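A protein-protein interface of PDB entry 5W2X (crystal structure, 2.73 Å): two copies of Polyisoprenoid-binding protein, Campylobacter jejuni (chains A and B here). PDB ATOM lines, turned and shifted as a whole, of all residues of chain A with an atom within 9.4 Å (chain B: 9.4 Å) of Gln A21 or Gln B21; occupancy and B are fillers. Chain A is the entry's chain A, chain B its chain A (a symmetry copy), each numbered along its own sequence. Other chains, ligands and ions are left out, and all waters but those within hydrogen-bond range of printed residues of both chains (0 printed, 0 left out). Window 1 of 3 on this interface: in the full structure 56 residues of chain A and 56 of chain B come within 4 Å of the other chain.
O of Thr A154 lies within hydrogen-bond range of N of Leu B20, 2.8 Å away. The backbone NH (N) of His B19 is in hydrogen-bond range of the backbone carbonyl oxygen (O) of Ser A23, at 2.8 Å. N of Leu A20 sits at hydrogen-bond distance from O of Thr B154, at 2.8 Å. The backbone NH (N) of Gln A21 sits at hydrogen-bond distance from the backbone carbonyl oxygen (O) of Gln B21 (2.9 Å). N of His A19 sits at hydrogen-bond distance from O of Ser B23, at 2.8 Å.
CA of Ile B22 touches O of His A19 (3.5 Å). Val B25 touches His A19. Gln B21 touches Leu A20 (O to CA, 3.5 Å). Leu A20 touches Ile B153 (CD1 to O, 3.6 Å). Gln A21 touches Leu B20 (O to CA, 3.5 Å). CA of Ile A22 touches O of His B19, 3.5 Å away. Leu B20 touches Ile A22. Leu B20 touches Ile A153 (CD1 to O, 3.6 Å). Thr A154 touches His B19. C of Leu A155 touches O of Lys B18, 3.7 Å away.
Of chain B, only His B19, Leu B20 and Gln B21 come within 4 Å of Gln A21. Of chain A, only His A19, Leu A20 and Gln A21 come within 4 Å of Gln B21. Printed residues of chain A within 4 Å of Asn B24: Lys A18 (3.2 Å). Of the printed residues of chain A, Ile B22 touches His A19 (3.5 Å) and Leu A20 (3.8 Å).
Printed residues of chain A that touch a printed residue of chain B: Lys A18, His A19, Leu A20, Gln A21, Ile A22, Ser A23, Asn A24, Val A25, Ile A153, Thr A154 and Leu A155. Printed residues of chain B that touch a printed residue of chain A: Lys B18, His B19, Leu B20, Gln B21, Ile B22, Ser B23, Asn B24, Val B25, Ile B153, Thr B154 and Leu B155. Hydrophobic or aromatic side chains of chain B within 4 Å of the printed part of chain A: His B19, Leu B20, Ile B22, Val B25, Ile B153 and Leu B155. Among the printed residues, 27 pairs touch across the chains. Among the printed residues, no Asp or Glu carboxylate lies within 4 Å of a Lys or Arg side-chain nitrogen of the other chain.
Lys A18 touches Ser B23, and with the chains exchanged Ser A23 touches Lys B18. Lys A18 touches Asn B24, and with the chains exchanged Asn A24 touches Lys B18. Lys A18 touches Leu B155, and with the chains exchanged Leu A155 touches Lys B18. His A19 touches Ser B23, and with the chains exchanged Ser A23 touches His B19. 13 positions are printed for both chains.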
ATOM      1  N   LYS A  18      21.275  28.264   4.999  1.00  0.00           N
ATOM      2  CA  LYS A  18      20.433  28.011   3.854  1.00  0.00           C
ATOM      3  C   LYS A  18      21.308  27.974   2.610  1.00  0.00           C
ATOM      4  O   LYS A  18      22.061  28.930   2.367  1.00  0.00           O
ATOM      5  CB  LYS A  18      19.382  29.128   3.730  1.00  0.00           C
ATOM      6  CG  LYS A  18      18.113  28.934   4.540  1.00  0.00           C
ATOM      7  CD  LYS A  18      17.412  30.276   4.705  1.00  0.00           C
ATOM      8  CE  LYS A  18      16.200  30.185   5.632  1.00  0.00           C
ATOM      9  NZ  LYS A  18      15.368  31.426   5.526  1.00  0.00           N
ATOM     10  N   HIS A  19      21.224  26.885   1.833  1.00  0.00           N
ATOM     11  CA  HIS A  19      21.760  26.892   0.453  1.00  0.00           C
ATOM     12  C   HIS A  19      20.810  26.427  -0.664  1.00  0.00           C
ATOM     13  O   HIS A  19      19.834  25.705  -0.419  1.00  0.00           O
ATOM     14  CB  HIS A  19      23.164  26.242   0.345  1.00  0.00           C
ATOM     15  CG  HIS A  19      23.177  24.744   0.210  1.00  0.00           C
ATOM     16  ND1 HIS A  19      22.242  23.916   0.812  1.00  0.00           N
ATOM     17  CD2 HIS A  19      24.059  23.924  -0.420  1.00  0.00           C
ATOM     18  CE1 HIS A  19      22.531  22.657   0.535  1.00  0.00           C
ATOM     19  NE2 HIS A  19      23.628  22.633  -0.211  1.00  0.00           N
ATOM     20  N   LEU A  20      21.122  26.885  -1.881  1.00  0.00           N
ATOM     21  CA  LEU A  20      20.470  26.467  -3.114  1.00  0.00           C
ATOM     22  C   LEU A  20      21.116  25.248  -3.724  1.00  0.00           C
ATOM     23  O   LEU A  20      22.329  25.096  -3.660  1.00  0.00           O
ATOM     24  CB  LEU A  20      20.527  27.595  -4.119  1.00  0.00           C
ATOM     25  CG  LEU A  20      19.674  28.788  -3.695  1.00  0.00           C
ATOM     26  CD1 LEU A  20      19.724  29.860  -4.776  1.00  0.00           C
ATOM     27  CD2 LEU A  20      18.234  28.372  -3.372  1.00  0.00           C
ATOM     28  N   GLN A  21      20.293  24.382  -4.309  1.00  0.00           N
ATOM     29  CA  GLN A  21      20.750  23.250  -5.118  1.00  0.00           C
ATOM     30  C   GLN A  21      19.956  23.144  -6.410  1.00  0.00           C
ATOM     31  O   GLN A  21      18.722  23.168  -6.405  1.00  0.00           O
ATOM     32  CB  GLN A  21      20.633  21.954  -4.347  1.00  0.00           C
ATOM     33  CG  GLN A  21      21.682  21.817  -3.275  1.00  0.00           C
ATOM     34  CD  GLN A  21      21.606  20.484  -2.574  1.00  0.00           C
ATOM     35  OE1 GLN A  21      20.592  20.148  -1.954  1.00  0.00           O
ATOM     36  NE2 GLN A  21      22.688  19.713  -2.660  1.00  0.00           N
ATOM     37  N   ILE A  22      20.683  23.037  -7.516  1.00  0.00           N
ATOM     38  CA  ILE A  22      20.104  22.862  -8.851  1.00  0.00           C
ATOM     39  C   ILE A  22      19.916  21.364  -9.109  1.00  0.00           C
ATOM     40  O   ILE A  22      20.752  20.558  -8.694  1.00  0.00           O
ATOM     41  CB  ILE A  22      20.993  23.546  -9.910  1.00  0.00           C
ATOM     42  CG1 ILE A  22      20.256  23.705 -11.243  1.00  0.00           C
ATOM     43  CG2 ILE A  22      22.349  22.849 -10.027  1.00  0.00           C
ATOM     44  CD1 ILE A  22      20.663  24.937 -12.045  1.00  0.00           C
ATOM     45  N   SER A  23      18.788  20.996  -9.722  1.00  0.00           N
ATOM     46  CA  SER A  23      18.501  19.600 -10.119  1.00  0.00           C
ATOM     47  C   SER A  23      17.600  19.540 -11.366  1.00  0.00           C
ATOM     48  O   SER A  23      16.781  20.444 -11.615  1.00  0.00           O
ATOM     49  CB  SER A  23      17.920  18.771  -8.959  1.00  0.00           C
ATOM     50  OG  SER A  23      16.546  19.061  -8.762  1.00  0.00           O
ATOM     51  N   ASN A  24      17.799  18.482 -12.159  1.00  0.00           N
ATOM     52  CA  ASN A  24      16.967  18.170 -13.322  1.00  0.00           C
ATOM     53  C   ASN A  24      15.715  17.464 -12.849  1.00  0.00           C
ATOM     54  O   ASN A  24      15.827  16.436 -12.181  1.00  0.00           O
ATOM     55  CB  ASN A  24      17.700  17.185 -14.247  1.00  0.00           C
ATOM     56  CG  ASN A  24      18.667  17.854 -15.202  1.00  0.00           C
ATOM     57  OD1 ASN A  24      18.515  19.028 -15.569  1.00  0.00           O
ATOM     58  ND2 ASN A  24      19.673  17.088 -15.634  1.00  0.00           N
ATOM     59  N   VAL A  25      14.536  17.986 -13.190  1.00  0.00           N
ATOM     60  CA  VAL A  25      13.340  17.134 -13.201  1.00  0.00           C
ATOM     61  C   VAL A  25      13.325  16.343 -14.526  1.00  0.00           C
ATOM     62  O   VAL A  25      13.319  16.953 -15.619  1.00  0.00           O
ATOM     63  CB  VAL A  25      12.026  17.919 -13.056  1.00  0.00           C
ATOM     64  CG1 VAL A  25      10.866  16.960 -12.818  1.00  0.00           C
ATOM     65  CG2 VAL A  25      12.105  18.879 -11.900  1.00  0.00           C
ATOM     66  N   ASN A  61       6.999  11.360  -8.934  1.00  0.00           N
ATOM     67  CA  ASN A  61       6.532  12.012  -7.730  1.00  0.00           C
ATOM     68  C   ASN A  61       5.035  12.220  -7.894  1.00  0.00           C
ATOM     69  O   ASN A  61       4.596  12.919  -8.810  1.00  0.00           O
ATOM     70  CB  ASN A  61       7.315  13.323  -7.542  1.00  0.00           C
ATOM     71  CG  ASN A  61       6.604  14.343  -6.665  1.00  0.00           C
ATOM     72  OD1 ASN A  61       5.369  14.430  -6.621  1.00  0.00           O
ATOM     73  ND2 ASN A  61       7.397  15.162  -5.992  1.00  0.00           N
ATOM     74  N   ARG A  64       3.561  16.158  -7.305  1.00  0.00           N
ATOM     75  CA  ARG A  64       3.998  17.168  -8.284  1.00  0.00           C
ATOM     76  C   ARG A  64       3.247  16.941  -9.586  1.00  0.00           C
ATOM     77  O   ARG A  64       2.850  17.889 -10.264  1.00  0.00           O
ATOM     78  CB  ARG A  64       5.501  17.146  -8.540  1.00  0.00           C
ATOM     79  CG  ARG A  64       6.082  18.496  -8.965  1.00  0.00           C
ATOM     80  CD  ARG A  64       7.134  18.313 -10.048  1.00  0.00           C
ATOM     81  NE  ARG A  64       8.437  17.863  -9.538  1.00  0.00           N
ATOM     82  CZ  ARG A  64       8.872  16.595  -9.544  1.00  0.00           C
ATOM     83  NH1 ARG A  64       8.111  15.619 -10.012  1.00  0.00           N
ATOM     84  NH2 ARG A  64      10.072  16.287  -9.065  1.00  0.00           N
ATOM     85  N   ILE A 153      14.028  31.963 -12.769  1.00  0.00           N
ATOM     86  CA  ILE A 153      15.008  31.574 -11.762  1.00  0.00           C
ATOM     87  C   ILE A 153      14.685  30.229 -11.097  1.00  0.00           C
ATOM     88  O   ILE A 153      15.494  29.308 -11.185  1.00  0.00           O
ATOM     89  CB  ILE A 153      15.195  32.641 -10.687  1.00  0.00           C
ATOM     90  CG1 ILE A 153      15.460  34.008 -11.329  1.00  0.00           C
ATOM     91  CG2 ILE A 153      16.359  32.251  -9.798  1.00  0.00           C
ATOM     92  CD1 ILE A 153      15.184  35.192 -10.410  1.00  0.00           C
ATOM     93  N   THR A 154      13.534  30.115 -10.432  1.00  0.00           N
ATOM     94  CA  THR A 154      13.118  28.867  -9.750  1.00  0.00           C
ATOM     95  C   THR A 154      13.184  27.637 -10.677  1.00  0.00           C
ATOM     96  O   THR A 154      13.763  26.598 -10.323  1.00  0.00           O
ATOM     97  CB  THR A 154      11.681  29.001  -9.172  1.00  0.00           C
ATOM     98  OG1 THR A 154      11.624  30.174  -8.359  1.00  0.00           O
ATOM     99  CG2 THR A 154      11.204  27.714  -8.360  1.00  0.00           C
ATOM    100  N   LEU A 155      12.572  27.793 -11.857  1.00  0.00           N
ATOM    101  CA  LEU A 155      12.395  26.742 -12.865  1.00  0.00           C
ATOM    102  C   LEU A 155      12.917  27.325 -14.142  1.00  0.00           C
ATOM    103  O   LEU A 155      12.606  28.484 -14.470  1.00  0.00           O
ATOM    104  CB  LEU A 155      10.936  26.456 -13.044  1.00  0.00           C
ATOM    105  CG  LEU A 155      10.481  25.345 -13.946  1.00  0.00           C
ATOM    106  CD1 LEU A 155      10.528  23.994 -13.247  1.00  0.00           C
ATOM    107  CD2 LEU A 155       9.048  25.673 -14.331  1.00  0.00           C
ATOM    108  N   LYS B  18      15.394  22.002 -15.534  1.00  0.00           N
ATOM    109  CA  LYS B  18      16.244  22.324 -14.413  1.00  0.00           C
ATOM    110  C   LYS B  18      15.464  23.213 -13.454  1.00  0.00           C
ATOM    111  O   LYS B  18      14.930  24.248 -13.882  1.00  0.00           O
ATOM    112  CB  LYS B  18      17.500  23.059 -14.911  1.00  0.00           C
ATOM    113  CG  LYS B  18      18.650  22.175 -15.359  1.00  0.00           C
ATOM    114  CD  LYS B  18      19.589  22.981 -16.247  1.00  0.00           C
ATOM    115  CE  LYS B  18      20.695  22.117 -16.853  1.00  0.00           C
ATOM    116  NZ  LYS B  18      21.760  22.982 -17.455  1.00  0.00           N
ATOM    117  N   HIS B  19      15.382  22.814 -12.176  1.00  0.00           N
ATOM    118  CA  HIS B  19      14.951  23.751 -11.114  1.00  0.00           C
ATOM    119  C   HIS B  19      15.863  23.872  -9.881  1.00  0.00           C
ATOM    120  O   HIS B  19      16.660  22.973  -9.580  1.00  0.00           O
ATOM    121  CB  HIS B  19      13.457  23.586 -10.732  1.00  0.00           C
ATOM    122  CG  HIS B  19      13.159  22.505  -9.729  1.00  0.00           C
ATOM    123  ND1 HIS B  19      13.871  21.318  -9.652  1.00  0.00           N
ATOM    124  CD2 HIS B  19      12.176  22.419  -8.794  1.00  0.00           C
ATOM    125  CE1 HIS B  19      13.359  20.563  -8.698  1.00  0.00           C
ATOM    126  NE2 HIS B  19      12.330  21.206  -8.160  1.00  0.00           N
ATOM    127  N   LEU B  20      15.728  25.016  -9.205  1.00  0.00           N
ATOM    128  CA  LEU B  20      16.365  25.301  -7.926  1.00  0.00           C
ATOM    129  C   LEU B  20      15.535  24.846  -6.753  1.00  0.00           C
ATOM    130  O   LEU B  20      14.313  24.927  -6.794  1.00  0.00           O
ATOM    131  CB  LEU B  20      16.598  26.789  -7.802  1.00  0.00           C
ATOM    132  CG  LEU B  20      17.639  27.295  -8.797  1.00  0.00           C
ATOM    133  CD1 LEU B  20      17.872  28.785  -8.580  1.00  0.00           C
ATOM    134  CD2 LEU B  20      18.945  26.495  -8.712  1.00  0.00           C
ATOM    135  N   GLN B  21      16.208  24.361  -5.713  1.00  0.00           N
ATOM    136  CA  GLN B  21      15.592  24.056  -4.420  1.00  0.00           C
ATOM    137  C   GLN B  21      16.433  24.590  -3.272  1.00  0.00           C
ATOM    138  O   GLN B  21      17.644  24.364  -3.209  1.00  0.00           O
ATOM    139  CB  GLN B  21      15.401  22.564  -4.253  1.00  0.00           C
ATOM    140  CG  GLN B  21      14.277  22.023  -5.096  1.00  0.00           C
ATOM    141  CD  GLN B  21      14.042  20.554  -4.854  1.00  0.00           C
ATOM    142  OE1 GLN B  21      14.927  19.723  -5.081  1.00  0.00           O
ATOM    143  NE2 GLN B  21      12.838  20.219  -4.395  1.00  0.00           N
ATOM    144  N   ILE B  22      15.775  25.312  -2.373  1.00  0.00           N
ATOM    145  CA  ILE B  22      16.395  25.860  -1.163  1.00  0.00           C
ATOM    146  C   ILE B  22      16.301  24.815  -0.049  1.00  0.00           C
ATOM    147  O   ILE B  22      15.297  24.104   0.047  1.00  0.00           O
ATOM    148  CB  ILE B  22      15.729  27.200  -0.787  1.00  0.00           C
ATOM    149  CG1 ILE B  22      16.570  27.976   0.232  1.00  0.00           C
ATOM    150  CG2 ILE B  22      14.274  26.996  -0.366  1.00  0.00           C
ATOM    151  CD1 ILE B  22      16.467  29.493   0.109  1.00  0.00           C
ATOM    152  N   SER B  23      17.373  24.674   0.735  1.00  0.00           N
ATOM    153  CA  SER B  23      17.405  23.770   1.906  1.00  0.00           C
ATOM    154  C   SER B  23      18.357  24.292   2.998  1.00  0.00           C
ATOM    155  O   SER B  23      19.353  24.982   2.710  1.00  0.00           O
ATOM    156  CB  SER B  23      17.734  22.318   1.515  1.00  0.00           C
ATOM    157  OG  SER B  23      19.122  22.155   1.275  1.00  0.00           O
ATOM    158  N   ASN B  24      18.008  23.985   4.251  1.00  0.00           N
ATOM    159  CA  ASN B  24      18.836  24.274   5.421  1.00  0.00           C
ATOM    160  C   ASN B  24      19.892  23.196   5.549  1.00  0.00           C
ATOM    161  O   ASN B  24      19.536  22.020   5.622  1.00  0.00           O
ATOM    162  CB  ASN B  24      17.988  24.206   6.701  1.00  0.00           C
ATOM    163  CG  ASN B  24      17.236  25.487   6.999  1.00  0.00           C
ATOM    164  OD1 ASN B  24      17.640  26.589   6.599  1.00  0.00           O
ATOM    165  ND2 ASN B  24      16.130  25.348   7.736  1.00  0.00           N
ATOM    166  N   VAL B  25      21.170  23.574   5.587  1.00  0.00           N
ATOM    167  CA  VAL B  25      22.173  22.684   6.184  1.00  0.00           C
ATOM    168  C   VAL B  25      22.120  22.859   7.717  1.00  0.00           C
ATOM    169  O   VAL B  25      22.318  23.985   8.225  1.00  0.00           O
ATOM    170  CB  VAL B  25      23.604  22.949   5.686  1.00  0.00           C
ATOM    171  CG1 VAL B  25      24.534  21.833   6.146  1.00  0.00           C
ATOM    172  CG2 VAL B  25      23.638  23.018   4.183  1.00  0.00           C
ATOM    173  N   ASN B  61      26.959  14.398   6.651  1.00  0.00           N
ATOM    174  CA  ASN B  61      27.464  14.092   5.330  1.00  0.00           C
ATOM    175  C   ASN B  61      28.981  14.059   5.436  1.00  0.00           C
ATOM    176  O   ASN B  61      29.608  15.063   5.779  1.00  0.00           O
ATOM    177  CB  ASN B  61      26.943  15.154   4.344  1.00  0.00           C
ATOM    178  CG  ASN B  61      27.782  15.281   3.080  1.00  0.00           C
ATOM    179  OD1 ASN B  61      29.004  15.080   3.075  1.00  0.00           O
ATOM    180  ND2 ASN B  61      27.122  15.670   2.000  1.00  0.00           N
ATOM    181  N   ARG B  64      31.158  16.476   2.707  1.00  0.00           N
ATOM    182  CA  ARG B  64      30.993  17.932   2.856  1.00  0.00           C
ATOM    183  C   ARG B  64      31.770  18.387   4.081  1.00  0.00           C
ATOM    184  O   ARG B  64      32.389  19.452   4.082  1.00  0.00           O
ATOM    185  CB  ARG B  64      29.535  18.364   2.974  1.00  0.00           C
ATOM    186  CG  ARG B  64      29.260  19.780   2.468  1.00  0.00           C
ATOM    187  CD  ARG B  64      28.267  20.494   3.372  1.00  0.00           C
ATOM    188  NE  ARG B  64      26.870  20.095   3.148  1.00  0.00           N
ATOM    189  CZ  ARG B  64      26.196  19.198   3.883  1.00  0.00           C
ATOM    190  NH1 ARG B  64      26.779  18.571   4.891  1.00  0.00           N
ATOM    191  NH2 ARG B  64      24.930  18.909   3.604  1.00  0.00           N
ATOM    192  N   ILE B 153      24.387  34.080  -3.077  1.00  0.00           N
ATOM    193  CA  ILE B 153      23.285  33.367  -3.714  1.00  0.00           C
ATOM    194  C   ILE B 153      23.292  31.861  -3.419  1.00  0.00           C
ATOM    195  O   ILE B 153      22.326  31.358  -2.851  1.00  0.00           O
ATOM    196  CB  ILE B 153      23.241  33.591  -5.223  1.00  0.00           C
ATOM    197  CG1 ILE B 153      23.293  35.089  -5.546  1.00  0.00           C
ATOM    198  CG2 ILE B 153      21.966  32.984  -5.776  1.00  0.00           C
ATOM    199  CD1 ILE B 153      23.735  35.404  -6.969  1.00  0.00           C
ATOM    200  N   THR B 154      24.352  31.149  -3.806  1.00  0.00           N
ATOM    201  CA  THR B 154      24.469  29.689  -3.576  1.00  0.00           C
ATOM    202  C   THR B 154      24.223  29.302  -2.105  1.00  0.00           C
ATOM    203  O   THR B 154      23.429  28.396  -1.804  1.00  0.00           O
ATOM    204  CB  THR B 154      25.862  29.165  -4.022  1.00  0.00           C
ATOM    205  OG1 THR B 154      26.095  29.580  -5.370  1.00  0.00           O
ATOM    206  CG2 THR B 154      26.022  27.586  -3.869  1.00  0.00           C
ATOM    207  N   LEU B 155      24.931  30.009  -1.214  1.00  0.00           N
ATOM    208  CA  LEU B 155      24.964  29.761   0.230  1.00  0.00           C
ATOM    209  C   LEU B 155      24.653  31.080   0.867  1.00  0.00           C
ATOM    210  O   LEU B 155      25.206  32.116   0.456  1.00  0.00           O
ATOM    211  CB  LEU B 155      26.347  29.359   0.641  1.00  0.00           C
ATOM    212  CG  LEU B 155      26.633  28.945   2.057  1.00  0.00           C
ATOM    213  CD1 LEU B 155      26.276  27.488   2.303  1.00  0.00           C
ATOM    214  CD2 LEU B 155      28.125  29.149   2.263  1.00  0.00           C
